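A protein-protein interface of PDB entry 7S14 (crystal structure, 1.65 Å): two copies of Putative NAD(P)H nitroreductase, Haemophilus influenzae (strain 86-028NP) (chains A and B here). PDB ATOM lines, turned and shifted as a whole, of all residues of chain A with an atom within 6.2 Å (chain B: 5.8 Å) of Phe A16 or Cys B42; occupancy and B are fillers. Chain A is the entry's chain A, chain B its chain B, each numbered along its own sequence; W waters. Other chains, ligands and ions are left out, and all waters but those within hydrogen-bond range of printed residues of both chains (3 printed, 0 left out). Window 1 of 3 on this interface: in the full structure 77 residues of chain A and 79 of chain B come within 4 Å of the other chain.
Printed residues of chain A that touch a printed residue of chain B: Val A12, Leu A13, Phe A16, His A17, Arg A19 and Thr A157.
Hydrophobic or aromatic side chains of chain A within 4 Å of the printed part of chain B: Val A12, Leu A13, Phe A16 and His A17.
Of the 16 printed residues of chain B, 5 touch a printed residue of chain A.
Hydrophobic or aromatic side chains of chain B that line the printed part of chain A: Leu B45.
Among the printed residues, 10 pairs touch across the chains.
Phe A16 touches three residues of chain B.
Of chain A, only Val A12 and Phe A16 come within 4 Å of Cys B42.
Printed residues of chain A within 4 Å of Cys B38: Val A12 and Leu A13.
Of the printed residues of chain A, Glu B41 touches Leu A13 (3.6 Å).
Printed residues of chain A within 4 Å of Asn B154: Phe A16 and Thr A157.
Of the printed residues of chain B, Leu A13 touches Cys B38 and Glu B41.
Printed residues of chain B within 4 Å of Thr A157: Asn B154.
The nearest residue of chain A that does not touch Cys B42 is Leu A13 (5.0 Å).
The nearest printed residue of chain A that does not touch Leu B45 is Leu A13 (4.7 Å).
OE1 of Glu B41 lies within salt-bridge range of NE of Arg B44, 2.5 Å away.
O of Cys B38 is in hydrogen-bond range of SG of Cys B42 (3.4 Å).
A ring nitrogen (ND1) of His A17 is in hydrogen-bond range of the side-chain amino group (NZ) of Lys A209.
O of Cys B42 sits at hydrogen-bond distance from OG of Ser B46 (3.0 Å).
OG of Ser B46 lies within hydrogen-bond range of ND2 of Asn B154 (3.0 Å).
Position printed for both chains: 157.
Of the 10 pairs that touch across the chains among the printed residues, none has its exchanged pair printed and touching as well.
Water W2 bridges OE2 of Glu B41 (2.6 Å) and NE2 of His A17 (2.9 Å).
Water W1 lies within hydrogen-bond range of the backbone carbonyl oxygen (O) of Leu B45 (2.7 Å), the backbone carbonyl oxygen (O) of Phe A16 (2.7 Å) and the guanidinium group (NE) of Arg A19 (2.8 Å).
Water W3 lies within hydrogen-bond range of ND2 of Asn B154 (2.7 Å) and OG1 of Thr A157 (3.3 Å).
Among the printed residues, pairs that only touch across the chains: Val A12 with Cys B38 (3.7 Å), Val A12 with Cys B42 (3.5 Å), Leu A13 with Cys B38 (3.7 Å), Leu A13 with Glu B41 (3.6 Å), Phe A16 with Cys B42 (3.4 Å), Phe A16 with Leu B45 (3.9 Å), Phe A16 with Asn B154 (3.6 Å), His A17 with Leu B45 (3.4 Å) and Arg A19 with Leu B45 (3.9 Å).
OG1 of Thr A157 lies within hydrogen-bond range of OD1 of Asn B154 (2.7 Å).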
ATOM      1  N   GLN A  11     -25.821 -11.008   5.295  1.00  0.00           N
ATOM      2  CA  GLN A  11     -25.165 -12.212   5.876  1.00  0.00           C
ATOM      3  C   GLN A  11     -25.228 -13.373   4.876  1.00  0.00           C
ATOM      4  O   GLN A  11     -24.239 -14.127   4.775  1.00  0.00           O
ATOM      5  CB  GLN A  11     -25.810 -12.582   7.210  1.00  0.00           C
ATOM      6  CG  GLN A  11     -25.425 -11.642   8.342  1.00  0.00           C
ATOM      7  CD  GLN A  11     -26.225 -11.895   9.595  1.00  0.00           C
ATOM      8  OE1 GLN A  11     -27.451 -12.010   9.564  1.00  0.00           O
ATOM      9  NE2 GLN A  11     -25.531 -11.979  10.717  1.00  0.00           N
ATOM     10  N   VAL A  12     -26.338 -13.505   4.148  1.00  0.00           N
ATOM     11  CA  VAL A  12     -26.537 -14.599   3.153  1.00  0.00           C
ATOM     12  C   VAL A  12     -25.584 -14.360   1.979  1.00  0.00           C
ATOM     13  O   VAL A  12     -24.903 -15.304   1.585  1.00  0.00           O
ATOM     14  CB  VAL A  12     -28.003 -14.696   2.696  1.00  0.00           C
ATOM     15  CG1 VAL A  12     -28.168 -15.678   1.544  1.00  0.00           C
ATOM     16  CG2 VAL A  12     -28.922 -15.066   3.848  1.00  0.00           C
ATOM     17  N   LEU A  13     -25.523 -13.134   1.458  1.00  0.00           N
ATOM     18  CA  LEU A  13     -24.717 -12.831   0.248  1.00  0.00           C
ATOM     19  C   LEU A  13     -23.223 -12.843   0.589  1.00  0.00           C
ATOM     20  O   LEU A  13     -22.443 -13.275  -0.276  1.00  0.00           O
ATOM     21  CB  LEU A  13     -25.180 -11.506  -0.361  1.00  0.00           C
ATOM     22  CG  LEU A  13     -26.601 -11.538  -0.925  1.00  0.00           C
ATOM     23  CD1 LEU A  13     -26.949 -10.233  -1.612  1.00  0.00           C
ATOM     24  CD2 LEU A  13     -26.779 -12.707  -1.884  1.00  0.00           C
ATOM     25  N   GLU A  14     -22.835 -12.421   1.797  1.00  0.00           N
ATOM     26  CA  GLU A  14     -21.423 -12.505   2.258  1.00  0.00           C
ATOM     27  C   GLU A  14     -21.020 -13.982   2.336  1.00  0.00           C
ATOM     28  O   GLU A  14     -19.870 -14.298   1.980  1.00  0.00           O
ATOM     29  CB  GLU A  14     -21.234 -11.789   3.594  1.00  0.00           C
ATOM     30  CG  GLU A  14     -21.216 -10.281   3.445  1.00  0.00           C
ATOM     31  CD  GLU A  14     -20.865  -9.515   4.706  1.00  0.00           C
ATOM     32  OE1 GLU A  14     -21.225  -9.976   5.811  1.00  0.00           O
ATOM     33  OE2 GLU A  14     -20.233  -8.457   4.576  1.00  0.00           O
ATOM     34  N   LEU A  15     -21.938 -14.853   2.762  1.00  0.00           N
ATOM     35  CA  LEU A  15     -21.691 -16.315   2.864  1.00  0.00           C
ATOM     36  C   LEU A  15     -21.445 -16.896   1.466  1.00  0.00           C
ATOM     37  O   LEU A  15     -20.408 -17.554   1.284  1.00  0.00           O
ATOM     38  CB  LEU A  15     -22.880 -16.996   3.547  1.00  0.00           C
ATOM     39  CG  LEU A  15     -22.791 -18.517   3.651  1.00  0.00           C
ATOM     40  CD1 LEU A  15     -21.472 -18.944   4.279  1.00  0.00           C
ATOM     41  CD2 LEU A  15     -23.967 -19.071   4.441  1.00  0.00           C
ATOM     42  N   PHE A  16     -22.349 -16.642   0.515  1.00  0.00           N
ATOM     43  CA  PHE A  16     -22.328 -17.249  -0.842  1.00  0.00           C
ATOM     44  C   PHE A  16     -21.247 -16.600  -1.717  1.00  0.00           C
ATOM     45  O   PHE A  16     -20.675 -17.321  -2.560  1.00  0.00           O
ATOM     46  CB  PHE A  16     -23.723 -17.229  -1.466  1.00  0.00           C
ATOM     47  CG  PHE A  16     -24.619 -18.312  -0.924  1.00  0.00           C
ATOM     48  CD1 PHE A  16     -24.338 -19.647  -1.176  1.00  0.00           C
ATOM     49  CD2 PHE A  16     -25.706 -18.007  -0.121  1.00  0.00           C
ATOM     50  CE1 PHE A  16     -25.139 -20.652  -0.655  1.00  0.00           C
ATOM     51  CE2 PHE A  16     -26.509 -19.014   0.394  1.00  0.00           C
ATOM     52  CZ  PHE A  16     -26.223 -20.332   0.130  1.00  0.00           C
ATOM     53  N   HIS A  17     -20.940 -15.313  -1.513  1.00  0.00           N
ATOM     54  CA  HIS A  17     -19.882 -14.600  -2.279  1.00  0.00           C
ATOM     55  C   HIS A  17     -18.494 -15.084  -1.848  1.00  0.00           C
ATOM     56  O   HIS A  17     -17.630 -15.209  -2.730  1.00  0.00           O
ATOM     57  CB  HIS A  17     -20.007 -13.076  -2.155  1.00  0.00           C
ATOM     58  CG  HIS A  17     -20.918 -12.475  -3.169  1.00  0.00           C
ATOM     59  ND1 HIS A  17     -20.517 -12.243  -4.471  1.00  0.00           N
ATOM     60  CD2 HIS A  17     -22.198 -12.057  -3.089  1.00  0.00           C
ATOM     61  CE1 HIS A  17     -21.515 -11.713  -5.149  1.00  0.00           C
ATOM     62  NE2 HIS A  17     -22.555 -11.584  -4.325  1.00  0.00           N
ATOM     63  N   GLN A  18     -18.286 -15.342  -0.551  1.00  0.00           N
ATOM     64  CA  GLN A  18     -16.942 -15.644   0.019  1.00  0.00           C
ATOM     65  C   GLN A  18     -16.578 -17.117  -0.212  1.00  0.00           C
ATOM     66  O   GLN A  18     -15.373 -17.421  -0.157  1.00  0.00           O
ATOM     67  CB  GLN A  18     -16.879 -15.304   1.511  1.00  0.00           C
ATOM     68  CG  GLN A  18     -17.166 -16.491   2.430  1.00  0.00           C
ATOM     69  CD  GLN A  18     -17.657 -16.098   3.803  1.00  0.00           C
ATOM     70  OE1 GLN A  18     -18.300 -15.068   3.983  1.00  0.00           O
ATOM     71  NE2 GLN A  18     -17.387 -16.941   4.787  1.00  0.00           N
ATOM     72  N   ARG A  19     -17.561 -18.006  -0.411  1.00  0.00           N
ATOM     73  CA  ARG A  19     -17.294 -19.449  -0.667  1.00  0.00           C
ATOM     74  C   ARG A  19     -16.665 -19.593  -2.055  1.00  0.00           C
ATOM     75  O   ARG A  19     -17.324 -19.238  -3.049  1.00  0.00           O
ATOM     76  CB  ARG A  19     -18.553 -20.319  -0.591  1.00  0.00           C
ATOM     77  CG  ARG A  19     -18.261 -21.807  -0.761  1.00  0.00           C
ATOM     78  CD  ARG A  19     -19.224 -22.521  -1.693  1.00  0.00           C
ATOM     79  NE  ARG A  19     -19.250 -21.881  -3.003  1.00  0.00           N
ATOM     80  CZ  ARG A  19     -18.510 -22.229  -4.051  1.00  0.00           C
ATOM     81  NH1 ARG A  19     -17.673 -23.252  -3.987  1.00  0.00           N
ATOM     82  NH2 ARG A  19     -18.630 -21.551  -5.180  1.00  0.00           N
ATOM     83  N   SER A  20     -15.436 -20.105  -2.113  1.00  0.00           N
ATOM     84  CA  SER A  20     -14.738 -20.451  -3.375  1.00  0.00           C
ATOM     85  C   SER A  20     -14.347 -21.929  -3.341  1.00  0.00           C
ATOM     86  O   SER A  20     -14.273 -22.526  -2.242  1.00  0.00           O
ATOM     87  CB  SER A  20     -13.548 -19.549  -3.620  1.00  0.00           C
ATOM     88  OG  SER A  20     -13.949 -18.329  -4.236  1.00  0.00           O
ATOM     89  N   THR A 157     -21.778 -25.569   1.432  1.00  0.00           N
ATOM     90  CA  THR A 157     -22.326 -24.337   2.060  1.00  0.00           C
ATOM     91  C   THR A 157     -22.129 -24.391   3.580  1.00  0.00           C
ATOM     92  O   THR A 157     -21.718 -23.361   4.149  1.00  0.00           O
ATOM     93  CB  THR A 157     -23.785 -24.115   1.647  1.00  0.00           C
ATOM     94  OG1 THR A 157     -23.766 -23.926   0.230  1.00  0.00           O
ATOM     95  CG2 THR A 157     -24.416 -22.926   2.337  1.00  0.00           C
ATOM     96  N   LYS A 209     -11.620 -14.978  -5.998  1.00  0.00           N
ATOM     97  CA  LYS A 209     -13.065 -15.127  -6.306  1.00  0.00           C
ATOM     98  C   LYS A 209     -13.210 -15.339  -7.817  1.00  0.00           C
ATOM     99  O   LYS A 209     -12.497 -14.654  -8.580  1.00  0.00           O
ATOM    100  CB  LYS A 209     -13.848 -13.899  -5.837  1.00  0.00           C
ATOM    101  CG  LYS A 209     -15.220 -13.736  -6.476  1.00  0.00           C
ATOM    102  CD  LYS A 209     -15.894 -12.430  -6.125  1.00  0.00           C
ATOM    103  CE  LYS A 209     -16.781 -12.537  -4.904  1.00  0.00           C
ATOM    104  NZ  LYS A 209     -17.964 -13.388  -5.170  1.00  0.00           N
ATOM    105  N   GLU B  37     -34.651 -11.475  -4.672  1.00  0.00           N
ATOM    106  CA  GLU B  37     -33.385 -11.233  -5.410  1.00  0.00           C
ATOM    107  C   GLU B  37     -32.252 -12.002  -4.718  1.00  0.00           C
ATOM    108  O   GLU B  37     -31.454 -12.635  -5.428  1.00  0.00           O
ATOM    109  CB  GLU B  37     -33.050  -9.747  -5.494  1.00  0.00           C
ATOM    110  CG  GLU B  37     -31.799  -9.477  -6.307  1.00  0.00           C
ATOM    111  CD  GLU B  37     -31.810  -8.194  -7.118  1.00  0.00           C
ATOM    112  OE1 GLU B  37     -32.857  -7.879  -7.725  1.00  0.00           O
ATOM    113  OE2 GLU B  37     -30.768  -7.511  -7.136  1.00  0.00           O
ATOM    114  N   CYS B  38     -32.193 -11.941  -3.384  1.00  0.00           N
ATOM    115  CA  CYS B  38     -31.168 -12.624  -2.549  1.00  0.00           C
ATOM    116  C   CYS B  38     -31.193 -14.130  -2.838  1.00  0.00           C
ATOM    117  O   CYS B  38     -30.125 -14.722  -3.113  1.00  0.00           O
ATOM    118  CB  CYS B  38     -31.413 -12.365  -1.069  1.00  0.00           C
ATOM    119  SG  CYS B  38     -30.011 -12.824  -0.024  1.00  0.00           S
ATOM    120  N   ILE B  39     -32.384 -14.722  -2.794  1.00  0.00           N
ATOM    121  CA  ILE B  39     -32.610 -16.165  -3.097  1.00  0.00           C
ATOM    122  C   ILE B  39     -32.018 -16.482  -4.478  1.00  0.00           C
ATOM    123  O   ILE B  39     -31.231 -17.452  -4.579  1.00  0.00           O
ATOM    124  CB  ILE B  39     -34.107 -16.504  -2.995  1.00  0.00           C
ATOM    125  CG1 ILE B  39     -34.580 -16.441  -1.539  1.00  0.00           C
ATOM    126  CG2 ILE B  39     -34.394 -17.855  -3.633  1.00  0.00           C
ATOM    127  CD1 ILE B  39     -36.075 -16.589  -1.361  1.00  0.00           C
ATOM    128  N   LEU B  40     -32.359 -15.694  -5.503  1.00  0.00           N
ATOM    129  CA  LEU B  40     -31.859 -15.911  -6.891  1.00  0.00           C
ATOM    130  C   LEU B  40     -30.328 -15.820  -6.921  1.00  0.00           C
ATOM    131  O   LEU B  40     -29.717 -16.601  -7.676  1.00  0.00           O
ATOM    132  CB  LEU B  40     -32.473 -14.903  -7.863  1.00  0.00           C
ATOM    133  CG  LEU B  40     -33.963 -15.059  -8.150  1.00  0.00           C
ATOM    134  CD1 LEU B  40     -34.461 -13.866  -8.942  1.00  0.00           C
ATOM    135  CD2 LEU B  40     -34.258 -16.360  -8.884  1.00  0.00           C
ATOM    136  N   GLU B  41     -29.728 -14.918  -6.135  1.00  0.00           N
ATOM    137  CA  GLU B  41     -28.250 -14.751  -6.077  1.00  0.00           C
ATOM    138  C   GLU B  41     -27.602 -16.026  -5.527  1.00  0.00           C
ATOM    139  O   GLU B  41     -26.528 -16.395  -6.028  1.00  0.00           O
ATOM    140  CB  GLU B  41     -27.853 -13.534  -5.242  1.00  0.00           C
ATOM    141  CG  GLU B  41     -28.150 -12.216  -5.926  1.00  0.00           C
ATOM    142  CD  GLU B  41     -27.126 -11.786  -6.963  1.00  0.00           C
ATOM    143  OE1 GLU B  41     -26.795 -12.602  -7.837  1.00  0.00           O
ATOM    144  OE2 GLU B  41     -26.667 -10.631  -6.895  1.00  0.00           O
ATOM    145  N   CYS B  42     -28.228 -16.689  -4.552  1.00  0.00           N
ATOM    146  CA  CYS B  42     -27.732 -17.978  -3.992  1.00  0.00           C
ATOM    147  C   CYS B  42     -27.598 -19.010  -5.116  1.00  0.00           C
ATOM    148  O   CYS B  42     -26.634 -19.798  -5.083  1.00  0.00           O
ATOM    149  CB  CYS B  42     -28.656 -18.509  -2.907  1.00  0.00           C
ATOM    150  SG  CYS B  42     -28.786 -17.376  -1.504  1.00  0.00           S
ATOM    151  N   GLY B  43     -28.545 -19.012  -6.056  1.00  0.00           N
ATOM    152  CA  GLY B  43     -28.516 -19.890  -7.242  1.00  0.00           C
ATOM    153  C   GLY B  43     -27.410 -19.463  -8.186  1.00  0.00           C
ATOM    154  O   GLY B  43     -26.593 -20.312  -8.598  1.00  0.00           O
ATOM    155  N   ARG B  44     -27.345 -18.167  -8.482  1.00  0.00           N
ATOM    156  CA  ARG B  44     -26.355 -17.601  -9.431  1.00  0.00           C
ATOM    157  C   ARG B  44     -24.934 -17.920  -8.960  1.00  0.00           C
ATOM    158  O   ARG B  44     -24.081 -18.252  -9.810  1.00  0.00           O
ATOM    159  CB  ARG B  44     -26.529 -16.088  -9.549  1.00  0.00           C
ATOM    160  CG  ARG B  44     -25.685 -15.492 -10.661  1.00  0.00           C
ATOM    161  CD  ARG B  44     -25.973 -14.027 -10.884  1.00  0.00           C
ATOM    162  NE  ARG B  44     -25.428 -13.210  -9.808  1.00  0.00           N
ATOM    163  CZ  ARG B  44     -24.195 -12.702  -9.758  1.00  0.00           C
ATOM    164  NH1 ARG B  44     -23.334 -12.898 -10.742  1.00  0.00           N
ATOM    165  NH2 ARG B  44     -23.827 -11.981  -8.713  1.00  0.00           N
ATOM    166  N   LEU B  45     -24.690 -17.805  -7.653  1.00  0.00           N
ATOM    167  CA  LEU B  45     -23.335 -17.845  -7.051  1.00  0.00           C
ATOM    168  C   LEU B  45     -22.914 -19.292  -6.797  1.00  0.00           C
ATOM    169  O   LEU B  45     -21.803 -19.495  -6.282  1.00  0.00           O
ATOM    170  CB  LEU B  45     -23.338 -17.039  -5.752  1.00  0.00           C
ATOM    171  CG  LEU B  45     -23.493 -15.533  -5.932  1.00  0.00           C
ATOM    172  CD1 LEU B  45     -23.477 -14.833  -4.585  1.00  0.00           C
ATOM    173  CD2 LEU B  45     -22.406 -14.976  -6.833  1.00  0.00           C
ATOM    174  N   SER B  46     -23.770 -20.260  -7.119  1.00  0.00           N
ATOM    175  CA  SER B  46     -23.486 -21.700  -6.899  1.00  0.00           C
ATOM    176  C   SER B  46     -22.260 -22.133  -7.697  1.00  0.00           C
ATOM    177  O   SER B  46     -22.004 -21.642  -8.799  1.00  0.00           O
ATOM    178  CB  SER B  46     -24.677 -22.543  -7.233  1.00  0.00           C
ATOM    179  OG  SER B  46     -25.650 -22.447  -6.212  1.00  0.00           O
ATOM    180  N   ALA B 151     -27.585 -25.372  -7.556  1.00  0.00           N
ATOM    181  CA  ALA B 151     -28.277 -24.059  -7.556  1.00  0.00           C
ATOM    182  C   ALA B 151     -29.602 -24.172  -6.792  1.00  0.00           C
ATOM    183  O   ALA B 151     -29.868 -23.306  -5.939  1.00  0.00           O
ATOM    184  CB  ALA B 151     -28.482 -23.553  -8.957  1.00  0.00           C
ATOM    185  N   ASN B 154     -28.955 -24.512  -2.913  1.00  0.00           N
ATOM    186  CA  ASN B 154     -28.480 -23.238  -2.313  1.00  0.00           C
ATOM    187  C   ASN B 154     -29.631 -22.227  -2.251  1.00  0.00           C
ATOM    188  O   ASN B 154     -29.665 -21.455  -1.282  1.00  0.00           O
ATOM    189  CB  ASN B 154     -27.222 -22.730  -3.014  1.00  0.00           C
ATOM    190  CG  ASN B 154     -26.005 -23.555  -2.648  1.00  0.00           C
ATOM    191  OD1 ASN B 154     -25.875 -24.018  -1.513  1.00  0.00           O
ATOM    192  ND2 ASN B 154     -25.107 -23.750  -3.595  1.00  0.00           N
ATOM    193  N   MET B 155     -30.566 -22.235  -3.202  1.00  0.00           N
ATOM    194  CA  MET B 155     -31.735 -21.315  -3.146  1.00  0.00           C
ATOM    195  C   MET B 155     -32.667 -21.716  -1.993  1.00  0.00           C
ATOM    196  O   MET B 155     -33.172 -20.797  -1.319  1.00  0.00           O
ATOM    197  CB  MET B 155     -32.438 -21.260  -4.502  1.00  0.00           C
ATOM    198  CG  MET B 155     -31.650 -20.473  -5.523  1.00  0.00           C
ATOM    199  SD  MET B 155     -32.735 -20.063  -7.094  1.00  0.00           S
ATOM    200  CE  MET B 155     -32.770 -21.785  -8.024  1.00  0.00           C
ATOM    201  N   THR B 157     -31.706 -23.128   0.825  1.00  0.00           N
ATOM    202  CA  THR B 157     -30.924 -22.774   2.040  1.00  0.00           C
ATOM    203  C   THR B 157     -30.948 -21.255   2.249  1.00  0.00           C
ATOM    204  O   THR B 157     -31.115 -20.822   3.403  1.00  0.00           O
ATOM    205  CB  THR B 157     -29.485 -23.293   1.958  1.00  0.00           C
ATOM    206  OG1 THR B 157     -29.554 -24.717   1.867  1.00  0.00           O
ATOM    207  CG2 THR B 157     -28.649 -22.880   3.149  1.00  0.00           C
ATOM    208  N   GLY B 158     -30.758 -20.483   1.179  1.00  0.00           N
ATOM    209  CA  GLY B 158     -30.875 -19.014   1.216  1.00  0.00           C
ATOM    210  C   GLY B 158     -32.249 -18.584   1.698  1.00  0.00           C
ATOM    211  O   GLY B 158     -32.332 -17.721   2.597  1.00  0.00           O
ATOM    212  N   ALA B 159     -33.309 -19.155   1.123  1.00  0.00           N
ATOM    213  CA  ALA B 159     -34.703 -18.895   1.548  1.00  0.00           C
ATOM    214  C   ALA B 159     -34.809 -19.192   3.048  1.00  0.00           C
ATOM    215  O   ALA B 159     -35.283 -18.314   3.793  1.00  0.00           O
ATOM    216  CB  ALA B 159     -35.671 -19.715   0.732  1.00  0.00           C
HETATM  217  O   HOH W   1     -20.977 -19.773  -3.726  1.00  0.00           O
HETATM  218  O   HOH W   2     -24.885 -10.012  -5.097  1.00  0.00           O
HETATM  219  O   HOH W   3     -23.065 -25.256  -2.652  1.00  0.00           O
